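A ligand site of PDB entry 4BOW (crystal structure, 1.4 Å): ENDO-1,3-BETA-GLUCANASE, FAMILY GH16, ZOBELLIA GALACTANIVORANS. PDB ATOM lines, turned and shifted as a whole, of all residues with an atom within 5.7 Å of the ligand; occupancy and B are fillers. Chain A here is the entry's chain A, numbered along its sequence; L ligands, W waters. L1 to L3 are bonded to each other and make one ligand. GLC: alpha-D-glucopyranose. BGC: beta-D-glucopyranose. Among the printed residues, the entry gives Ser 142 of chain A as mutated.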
ATOM      1  N   TRP A  42      32.645 -37.150   4.071  1.00  0.00           N
ATOM      2  CA  TRP A  42      31.979 -36.003   4.777  1.00  0.00           C
ATOM      3  C   TRP A  42      30.479 -36.091   4.504  1.00  0.00           C
ATOM      4  O   TRP A  42      30.011 -37.026   3.765  1.00  0.00           O
ATOM      5  CB  TRP A  42      32.673 -34.679   4.331  1.00  0.00           C
ATOM      6  CG  TRP A  42      33.982 -34.654   5.059  1.00  0.00           C
ATOM      7  CD1 TRP A  42      35.194 -35.225   4.628  1.00  0.00           C
ATOM      8  CD2 TRP A  42      34.209 -34.172   6.398  1.00  0.00           C
ATOM      9  NE1 TRP A  42      36.154 -35.079   5.646  1.00  0.00           N
ATOM     10  CE2 TRP A  42      35.564 -34.479   6.738  1.00  0.00           C
ATOM     11  CE3 TRP A  42      33.386 -33.496   7.316  1.00  0.00           C
ATOM     12  CZ2 TRP A  42      36.085 -34.162   8.000  1.00  0.00           C
ATOM     13  CZ3 TRP A  42      33.892 -33.192   8.565  1.00  0.00           C
ATOM     14  CH2 TRP A  42      35.225 -33.546   8.901  1.00  0.00           C
ATOM     15  N   HIS A  43      29.758 -35.150   5.090  1.00  0.00           N
ATOM     16  CA  HIS A  43      28.282 -35.154   4.909  1.00  0.00           C
ATOM     17  C   HIS A  43      27.872 -34.451   3.622  1.00  0.00           C
ATOM     18  O   HIS A  43      28.724 -33.994   2.833  1.00  0.00           O
ATOM     19  CB  HIS A  43      27.647 -34.395   6.082  1.00  0.00           C
ATOM     20  CG  HIS A  43      27.995 -34.987   7.414  1.00  0.00           C
ATOM     21  ND1 HIS A  43      27.526 -36.220   7.795  1.00  0.00           N
ATOM     22  CD2 HIS A  43      28.743 -34.482   8.443  1.00  0.00           C
ATOM     23  CE1 HIS A  43      27.918 -36.454   9.057  1.00  0.00           C
ATOM     24  NE2 HIS A  43      28.676 -35.391   9.461  1.00  0.00           N
ATOM     25  N   ASN A  44      26.573 -34.379   3.353  1.00  0.00           N
ATOM     26  CA  ASN A  44      26.052 -33.591   2.267  1.00  0.00           C
ATOM     27  C   ASN A  44      26.501 -34.065   0.872  1.00  0.00           C
ATOM     28  O   ASN A  44      26.490 -33.306  -0.052  1.00  0.00           O
ATOM     29  CB  ASN A  44      26.344 -32.062   2.467  1.00  0.00           C
ATOM     30  CG  ASN A  44      25.994 -31.600   3.848  1.00  0.00           C
ATOM     31  OD1 ASN A  44      24.907 -31.859   4.357  1.00  0.00           O
ATOM     32  ND2 ASN A  44      26.907 -30.952   4.462  1.00  0.00           N
ATOM     33  N   GLU A  46      29.362 -34.465  -0.071  1.00  0.00           N
ATOM     34  CA  GLU A  46      30.535 -33.676  -0.509  1.00  0.00           C
ATOM     35  C   GLU A  46      31.635 -34.623  -0.997  1.00  0.00           C
ATOM     36  O   GLU A  46      31.758 -35.791  -0.579  1.00  0.00           O
ATOM     37  CB  GLU A  46      31.118 -32.956   0.729  1.00  0.00           C
ATOM     38  CG  GLU A  46      30.141 -31.836   1.180  1.00  0.00           C
ATOM     39  CD  GLU A  46      30.429 -31.331   2.596  1.00  0.00           C
ATOM     40  OE1 GLU A  46      31.504 -31.620   3.152  1.00  0.00           O
ATOM     41  OE2 GLU A  46      29.497 -30.633   3.107  1.00  0.00           O
ATOM     42  N   ARG A  86      39.441 -27.863   6.681  1.00  0.00           N
ATOM     43  CA  ARG A  86      38.301 -27.562   7.553  1.00  0.00           C
ATOM     44  C   ARG A  86      38.960 -27.299   8.899  1.00  0.00           C
ATOM     45  O   ARG A  86      39.420 -28.212   9.617  1.00  0.00           O
ATOM     46  CB  ARG A  86      37.336 -28.766   7.557  1.00  0.00           C
ATOM     47  CG  ARG A  86      36.143 -28.504   8.591  1.00  0.00           C
ATOM     48  CD  ARG A  86      35.081 -29.576   8.237  1.00  0.00           C
ATOM     49  NE  ARG A  86      34.048 -29.668   9.257  1.00  0.00           N
ATOM     50  CZ  ARG A  86      32.770 -29.919   9.032  1.00  0.00           C
ATOM     51  NH1 ARG A  86      32.268 -29.920   7.784  1.00  0.00           N
ATOM     52  NH2 ARG A  86      31.981 -30.147  10.066  1.00  0.00           N
ATOM     53  N   TRP A 111      32.142 -24.631  -2.323  1.00  0.00           N
ATOM     54  CA  TRP A 111      31.133 -24.347  -1.279  1.00  0.00           C
ATOM     55  C   TRP A 111      31.895 -23.880  -0.010  1.00  0.00           C
ATOM     56  O   TRP A 111      32.162 -24.694   0.901  1.00  0.00           O
ATOM     57  CB  TRP A 111      30.341 -25.604  -1.055  1.00  0.00           C
ATOM     58  CG  TRP A 111      29.298 -25.548   0.019  1.00  0.00           C
ATOM     59  CD1 TRP A 111      28.828 -24.471   0.744  1.00  0.00           C
ATOM     60  CD2 TRP A 111      28.535 -26.695   0.449  1.00  0.00           C
ATOM     61  NE1 TRP A 111      27.874 -24.872   1.648  1.00  0.00           N
ATOM     62  CE2 TRP A 111      27.695 -26.229   1.529  1.00  0.00           C
ATOM     63  CE3 TRP A 111      28.529 -28.044   0.124  1.00  0.00           C
ATOM     64  CZ2 TRP A 111      26.806 -27.072   2.164  1.00  0.00           C
ATOM     65  CZ3 TRP A 111      27.600 -28.875   0.756  1.00  0.00           C
ATOM     66  CH2 TRP A 111      26.778 -28.430   1.785  1.00  0.00           C
ATOM     67  N   PRO A 112      32.270 -22.605   0.028  1.00  0.00           N
ATOM     68  CA  PRO A 112      32.953 -22.061   1.226  1.00  0.00           C
ATOM     69  C   PRO A 112      31.943 -21.843   2.343  1.00  0.00           C
ATOM     70  O   PRO A 112      30.722 -21.593   2.065  1.00  0.00           O
ATOM     71  CB  PRO A 112      33.472 -20.721   0.708  1.00  0.00           C
ATOM     72  CG  PRO A 112      32.406 -20.229  -0.278  1.00  0.00           C
ATOM     73  CD  PRO A 112      32.025 -21.578  -1.023  1.00  0.00           C
ATOM     74  N   ALA A 113      32.409 -21.867   3.597  1.00  0.00           N
ATOM     75  CA  ALA A 113      31.571 -21.505   4.694  1.00  0.00           C
ATOM     76  C   ALA A 113      32.367 -20.976   5.843  1.00  0.00           C
ATOM     77  O   ALA A 113      33.516 -21.353   6.104  1.00  0.00           O
ATOM     78  CB  ALA A 113      30.745 -22.771   5.141  1.00  0.00           C
ATOM     79  N   TRP A 115      31.025 -20.667   9.773  1.00  0.00           N
ATOM     80  CA  TRP A 115      29.849 -21.098  10.518  1.00  0.00           C
ATOM     81  C   TRP A 115      30.243 -21.528  11.914  1.00  0.00           C
ATOM     82  O   TRP A 115      31.425 -21.503  12.282  1.00  0.00           O
ATOM     83  CB  TRP A 115      29.124 -22.200   9.704  1.00  0.00           C
ATOM     84  CG  TRP A 115      29.913 -23.418   9.312  1.00  0.00           C
ATOM     85  CD1 TRP A 115      31.057 -23.488   8.531  1.00  0.00           C
ATOM     86  CD2 TRP A 115      29.566 -24.762   9.630  1.00  0.00           C
ATOM     87  NE1 TRP A 115      31.416 -24.835   8.330  1.00  0.00           N
ATOM     88  CE2 TRP A 115      30.548 -25.608   8.998  1.00  0.00           C
ATOM     89  CE3 TRP A 115      28.525 -25.357  10.400  1.00  0.00           C
ATOM     90  CZ2 TRP A 115      30.468 -27.023   9.040  1.00  0.00           C
ATOM     91  CZ3 TRP A 115      28.467 -26.767  10.442  1.00  0.00           C
ATOM     92  CH2 TRP A 115      29.409 -27.595   9.788  1.00  0.00           C
ATOM     93  N   LEU A 117      29.287 -24.455  15.283  1.00  0.00           N
ATOM     94  CA  LEU A 117      28.613 -25.623  15.835  1.00  0.00           C
ATOM     95  C   LEU A 117      28.606 -25.443  17.327  1.00  0.00           C
ATOM     96  O   LEU A 117      29.592 -24.988  17.940  1.00  0.00           O
ATOM     97  CB  LEU A 117      29.331 -26.961  15.536  1.00  0.00           C
ATOM     98  CG  LEU A 117      29.072 -27.491  14.140  1.00  0.00           C
ATOM     99  CD1 LEU A 117      30.089 -28.611  13.856  1.00  0.00           C
ATOM    100  CD2 LEU A 117      27.578 -27.962  14.073  1.00  0.00           C
ATOM    101  N   GLU A 123      31.304 -33.850  17.298  1.00  0.00           N
ATOM    102  CA  GLU A 123      31.547 -34.318  15.958  1.00  0.00           C
ATOM    103  C   GLU A 123      32.862 -35.077  15.983  1.00  0.00           C
ATOM    104  O   GLU A 123      33.838 -34.678  16.610  1.00  0.00           O
ATOM    105  CB  GLU A 123      31.592 -33.090  15.012  1.00  0.00           C
ATOM    106  CG  GLU A 123      32.070 -33.531  13.626  1.00  0.00           C
ATOM    107  CD  GLU A 123      31.702 -32.487  12.625  1.00  0.00           C
ATOM    108  OE1 GLU A 123      30.570 -32.568  12.019  1.00  0.00           O
ATOM    109  OE2 GLU A 123      32.501 -31.574  12.386  1.00  0.00           O
ATOM    110  N   GLU A 136      24.063 -34.684  19.339  1.00  0.00           N
ATOM    111  CA  GLU A 136      24.333 -34.900  17.904  1.00  0.00           C
ATOM    112  C   GLU A 136      23.553 -33.889  17.082  1.00  0.00           C
ATOM    113  O   GLU A 136      22.384 -33.578  17.311  1.00  0.00           O
ATOM    114  CB  GLU A 136      23.892 -36.322  17.501  1.00  0.00           C
ATOM    115  CG  GLU A 136      24.328 -36.665  16.047  1.00  0.00           C
ATOM    116  CD  GLU A 136      24.061 -38.097  15.698  1.00  0.00           C
ATOM    117  OE1 GLU A 136      23.339 -38.757  16.466  1.00  0.00           O
ATOM    118  OE2 GLU A 136      24.589 -38.544  14.656  1.00  0.00           O
ATOM    119  N   TRP A 137      24.266 -33.366  16.076  1.00  0.00           N
ATOM    120  CA  TRP A 137      23.663 -32.348  15.186  1.00  0.00           C
ATOM    121  C   TRP A 137      22.325 -32.897  14.692  1.00  0.00           C
ATOM    122  O   TRP A 137      22.204 -34.070  14.323  1.00  0.00           O
ATOM    123  CB  TRP A 137      24.632 -32.053  14.030  1.00  0.00           C
ATOM    124  CG  TRP A 137      24.171 -30.982  13.058  1.00  0.00           C
ATOM    125  CD1 TRP A 137      24.578 -29.627  13.058  1.00  0.00           C
ATOM    126  CD2 TRP A 137      23.188 -31.149  11.992  1.00  0.00           C
ATOM    127  NE1 TRP A 137      23.945 -28.989  11.994  1.00  0.00           N
ATOM    128  CE2 TRP A 137      23.080 -29.887  11.372  1.00  0.00           C
ATOM    129  CE3 TRP A 137      22.417 -32.244  11.493  1.00  0.00           C
ATOM    130  CZ2 TRP A 137      22.257 -29.709  10.208  1.00  0.00           C
ATOM    131  CZ3 TRP A 137      21.639 -32.054  10.393  1.00  0.00           C
ATOM    132  CH2 TRP A 137      21.495 -30.809   9.824  1.00  0.00           C
ATOM    133  N   PRO A 138      21.243 -32.075  14.676  1.00  0.00           N
ATOM    134  CA  PRO A 138      21.244 -30.621  14.847  1.00  0.00           C
ATOM    135  C   PRO A 138      20.989 -30.188  16.271  1.00  0.00           C
ATOM    136  O   PRO A 138      20.863 -28.974  16.488  1.00  0.00           O
ATOM    137  CB  PRO A 138      20.091 -30.184  13.904  1.00  0.00           C
ATOM    138  CG  PRO A 138      19.033 -31.308  14.106  1.00  0.00           C
ATOM    139  CD  PRO A 138      19.930 -32.559  14.128  1.00  0.00           C
ATOM    140  N   SER A 142      23.662 -24.850  15.078  1.00  0.00           N
ATOM    141  CA  SER A 142      24.614 -24.218  14.234  1.00  0.00           C
ATOM    142  C   SER A 142      24.146 -22.923  13.651  1.00  0.00           C
ATOM    143  O   SER A 142      22.965 -22.766  13.358  1.00  0.00           O
ATOM    144  CB  SER A 142      24.734 -25.260  13.195  1.00  0.00           C
ATOM    145  OG  SER A 142      25.637 -24.846  12.162  1.00  0.00           O
ATOM    146  N   ASP A 144      25.096 -20.413  10.402  1.00  0.00           N
ATOM    147  CA  ASP A 144      25.923 -20.121   9.207  1.00  0.00           C
ATOM    148  C   ASP A 144      26.095 -18.643   9.027  1.00  0.00           C
ATOM    149  O   ASP A 144      25.066 -17.987   8.575  1.00  0.00           O
ATOM    150  CB  ASP A 144      25.257 -20.766   7.939  1.00  0.00           C
ATOM    151  CG  ASP A 144      25.263 -22.266   8.039  1.00  0.00           C
ATOM    152  OD1 ASP A 144      26.356 -22.827   7.975  1.00  0.00           O
ATOM    153  OD2 ASP A 144      24.279 -22.964   7.904  1.00  0.00           O
ATOM    154  N   GLU A 147      27.662 -18.790   3.704  1.00  0.00           N
ATOM    155  CA  GLU A 147      27.888 -19.871   2.726  1.00  0.00           C
ATOM    156  C   GLU A 147      27.689 -19.288   1.364  1.00  0.00           C
ATOM    157  O   GLU A 147      26.970 -18.322   1.170  1.00  0.00           O
ATOM    158  CB  GLU A 147      26.987 -21.080   2.860  1.00  0.00           C
ATOM    159  CG  GLU A 147      27.006 -21.675   4.278  1.00  0.00           C
ATOM    160  CD  GLU A 147      25.983 -22.783   4.301  1.00  0.00           C
ATOM    161  OE1 GLU A 147      26.114 -23.927   3.800  1.00  0.00           O
ATOM    162  OE2 GLU A 147      24.777 -22.624   4.863  1.00  0.00           O
ATOM    163  N   HIS A 161      20.541 -23.941  11.721  1.00  0.00           N
ATOM    164  CA  HIS A 161      20.098 -25.271  11.777  1.00  0.00           C
ATOM    165  C   HIS A 161      20.044 -25.705  13.228  1.00  0.00           C
ATOM    166  O   HIS A 161      21.081 -25.603  13.914  1.00  0.00           O
ATOM    167  CB  HIS A 161      21.051 -26.258  11.035  1.00  0.00           C
ATOM    168  CG  HIS A 161      21.214 -25.919   9.551  1.00  0.00           C
ATOM    169  ND1 HIS A 161      22.063 -24.906   9.129  1.00  0.00           N
ATOM    170  CD2 HIS A 161      20.635 -26.448   8.454  1.00  0.00           C
ATOM    171  CE1 HIS A 161      21.975 -24.861   7.758  1.00  0.00           C
ATOM    172  NE2 HIS A 161      21.099 -25.769   7.378  1.00  0.00           N
ATOM    173  N   TYR A 170      13.553 -30.891  13.553  1.00  0.00           N
ATOM    174  CA  TYR A 170      14.687 -30.249  12.961  1.00  0.00           C
ATOM    175  C   TYR A 170      14.190 -28.998  12.270  1.00  0.00           C
ATOM    176  O   TYR A 170      13.272 -29.108  11.441  1.00  0.00           O
ATOM    177  CB  TYR A 170      15.420 -31.198  11.988  1.00  0.00           C
ATOM    178  CG  TYR A 170      16.361 -30.530  10.977  1.00  0.00           C
ATOM    179  CD1 TYR A 170      17.394 -29.661  11.412  1.00  0.00           C
ATOM    180  CD2 TYR A 170      16.257 -30.834   9.592  1.00  0.00           C
ATOM    181  CE1 TYR A 170      18.264 -29.076  10.518  1.00  0.00           C
ATOM    182  CE2 TYR A 170      17.140 -30.273   8.624  1.00  0.00           C
ATOM    183  CZ  TYR A 170      18.128 -29.422   9.121  1.00  0.00           C
ATOM    184  OH  TYR A 170      19.013 -28.837   8.246  1.00  0.00           O
ATOM    185  N   ASN A 227      35.886 -23.460   6.048  1.00  0.00           N
ATOM    186  CA  ASN A 227      36.175 -24.604   5.147  1.00  0.00           C
ATOM    187  C   ASN A 227      35.807 -24.229   3.730  1.00  0.00           C
ATOM    188  O   ASN A 227      35.035 -23.278   3.493  1.00  0.00           O
ATOM    189  CB  ASN A 227      35.443 -25.927   5.554  1.00  0.00           C
ATOM    190  CG  ASN A 227      33.957 -25.728   5.424  1.00  0.00           C
ATOM    191  OD1 ASN A 227      33.321 -25.073   6.252  1.00  0.00           O
ATOM    192  ND2 ASN A 227      33.400 -26.271   4.352  1.00  0.00           N
HETATM  193  C1  GLC L   1      25.322 -25.768   7.130  1.00  0.00           C
HETATM  194  C2  GLC L   1      25.076 -27.250   7.017  1.00  0.00           C
HETATM  195  C3  GLC L   1      26.310 -28.134   7.262  1.00  0.00           C
HETATM  196  C4  GLC L   1      27.355 -27.597   6.301  1.00  0.00           C
HETATM  197  C5  GLC L   1      27.676 -26.226   6.793  1.00  0.00           C
HETATM  198  C6  GLC L   1      28.829 -25.503   6.036  1.00  0.00           C
HETATM  199  O1  GLC L   1      25.578 -25.467   8.499  1.00  0.00           O
HETATM  200  O2  GLC L   1      24.031 -27.554   7.932  1.00  0.00           O
HETATM  201  O3  GLC L   1      26.039 -29.545   6.984  1.00  0.00           O
HETATM  202  O4  GLC L   1      28.510 -28.403   6.474  1.00  0.00           O
HETATM  203  O5  GLC L   1      26.528 -25.377   6.549  1.00  0.00           O
HETATM  204  O6  GLC L   1      28.485 -25.388   4.599  1.00  0.00           O
HETATM  205  C2  BGC L   2      25.300 -31.679   7.692  1.00  0.00           C
HETATM  206  C3  BGC L   2      25.086 -32.512   8.901  1.00  0.00           C
HETATM  207  C4  BGC L   2      26.307 -32.491   9.849  1.00  0.00           C
HETATM  208  C5  BGC L   2      26.566 -31.014  10.269  1.00  0.00           C
HETATM  209  C6  BGC L   2      27.821 -30.834  11.099  1.00  0.00           C
HETATM  210  C1  BGC L   2      25.696 -30.295   8.182  1.00  0.00           C
HETATM  211  O2  BGC L   2      24.145 -31.580   6.918  1.00  0.00           O
HETATM  212  O3  BGC L   2      25.013 -33.904   8.429  1.00  0.00           O
HETATM  213  O4  BGC L   2      26.040 -33.170  11.097  1.00  0.00           O
HETATM  214  O5  BGC L   2      26.851 -30.336   9.009  1.00  0.00           O
HETATM  215  O6  BGC L   2      29.011 -31.330  10.388  1.00  0.00           O
HETATM  216  C2  BGC L   3      23.581 -35.784   7.966  1.00  0.00           C
HETATM  217  C3  BGC L   3      22.583 -36.687   8.709  1.00  0.00           C
HETATM  218  C4  BGC L   3      23.178 -37.239   9.977  1.00  0.00           C
HETATM  219  C5  BGC L   3      23.562 -36.066  10.894  1.00  0.00           C
HETATM  220  C6  BGC L   3      24.384 -36.516  12.090  1.00  0.00           C
HETATM  221  C1  BGC L   3      23.899 -34.674   8.996  1.00  0.00           C
HETATM  222  O2  BGC L   3      22.957 -35.172   6.871  1.00  0.00           O
HETATM  223  O3  BGC L   3      22.233 -37.727   7.824  1.00  0.00           O
HETATM  224  O4  BGC L   3      22.194 -37.920  10.763  1.00  0.00           O
HETATM  225  O5  BGC L   3      24.479 -35.253  10.160  1.00  0.00           O
HETATM  226  O6  BGC L   3      24.434 -35.338  12.872  1.00  0.00           O
HETATM  227  O   HOH W   1      30.724 -25.863   3.171  1.00  0.00           O
HETATM  228  O   HOH W   2      29.472 -30.641   7.708  1.00  0.00           O
HETATM  229  O   HOH W   3      22.492 -29.350   6.594  1.00  0.00           O
HETATM  230  O   HOH W   4      24.514 -26.819  10.517  1.00  0.00           O
HETATM  231  O   HOH W   5      24.461 -35.522   4.774  1.00  0.00           O
HETATM  232  O   HOH W   6      27.163 -35.163  13.582  1.00  0.00           O
HETATM  233  O   HOH W   7      21.227 -32.840   6.633  1.00  0.00           O
HETATM  234  O   HOH W   8      23.830 -23.351  10.582  1.00  0.00           O
HETATM  235  O   HOH W   9      30.165 -28.321   4.290  1.00  0.00           O
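The indole nitrogen (NE1) of Trp 111 lies within hydrogen-bond range of an oxygen (O6) of GLC L1 (3.1 Å). OD1 of Asn 44 lies within hydrogen-bond range of O2 of BGC L2, 2.7 Å away. An oxygen (O6) of BGC L2 lies within hydrogen-bond range of the guanidinium group of Arg 86, 3.2 Å away. The side-chain carboxylate of Glu 147 lies within hydrogen-bond range of an oxygen (O6) of GLC L1, at 2.9 Å. O2 of GLC L1 lies close to NE2 of His 161, at 3.5 Å. An oxygen (O6) of BGC L2 lies within hydrogen-bond range of the side-chain carboxylate (OE1) of Glu 123, at 2.6 Å. The backbone carbonyl oxygen (O) of Trp 137 is in hydrogen-bond range of an oxygen (O6) of BGC L3 (2.9 Å). OD1 of Asp 144 lies within hydrogen-bond range of O1 of GLC L1. A ring nitrogen (ND1) of His 43 sits close to an oxygen (O3) of BGC L2 (3.5 Å).
Residues that only touch the ligand: Glu 136, Trp 115, Ala 113 and Ser 142. Hydrophobic or aromatic side chains that line the ligand: His 43, Trp 111, Ala 113, Trp 115, Trp 137 and His 161. 13 residues have an atom within 4 Å of the ligand: His 43, Asn 44, Arg 86, Trp 111, Ala 113, Trp 115, Glu 123, Glu 136, Trp 137, Ser 142, Asp 144, Glu 147 and His 161. The nearest printed residue that does not touch the ligand is Leu 117 (4.1 Å).
OD2 of Asp 144 lies close to ND1 of His 161 (3.2 Å). The side-chain carboxylate (OE2) of Glu 123 is in salt-bridge range of the guanidinium group (NH2) of Arg 86, 2.8 Å away. NE1 of Trp 115 is in hydrogen-bond range of OD1 of Asn 227 (2.8 Å). N of Ser 142 lies within hydrogen-bond range of O of His 161, 2.9 Å away. The side-chain carboxylate (OE2) of Glu 46 is in hydrogen-bond range of the side-chain amide nitrogen (ND2) of Asn 44, at 2.9 Å. N of Ala 113 lies within hydrogen-bond range of O of Asn 227, 3.0 Å away. The side-chain carboxylate (OE1) of Glu 147 sits at hydrogen-bond distance from the indole nitrogen (NE1) of Trp 111 (2.9 Å).
Water W5 lies within hydrogen-bond range of an oxygen (O2) of BGC L3 (2.6 Å) and the backbone NH (N) of Asn 44 (2.8 Å). Water W4 lies within hydrogen-bond range of an oxygen (O1) of GLC L1 (2.7 Å), the indole nitrogen (NE1) of Trp 137 (2.7 Å), the side-chain hydroxyl (OG) of Ser 142 (2.8 Å) and a ring nitrogen (ND1) of His 161 (3.4 Å). Water W1 lies within hydrogen-bond range of O6 of GLC L1, O of Trp 111 and ND2 of Asn 227. Water W2 bridges O4 of GLC L1 (2.7 Å) and NH1 of Arg 86 (2.9 Å). Water W9 lies within hydrogen-bond range of OE2 of Glu 46 (2.7 Å) and O4 of GLC L1 (2.7 Å). Water W8 lies within hydrogen-bond range of the side-chain carboxylate (OD2) of Asp 144, a ring nitrogen (ND1) of His 161, the side-chain hydroxyl (OG) of Ser 142 and an oxygen (O1) of GLC L1.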
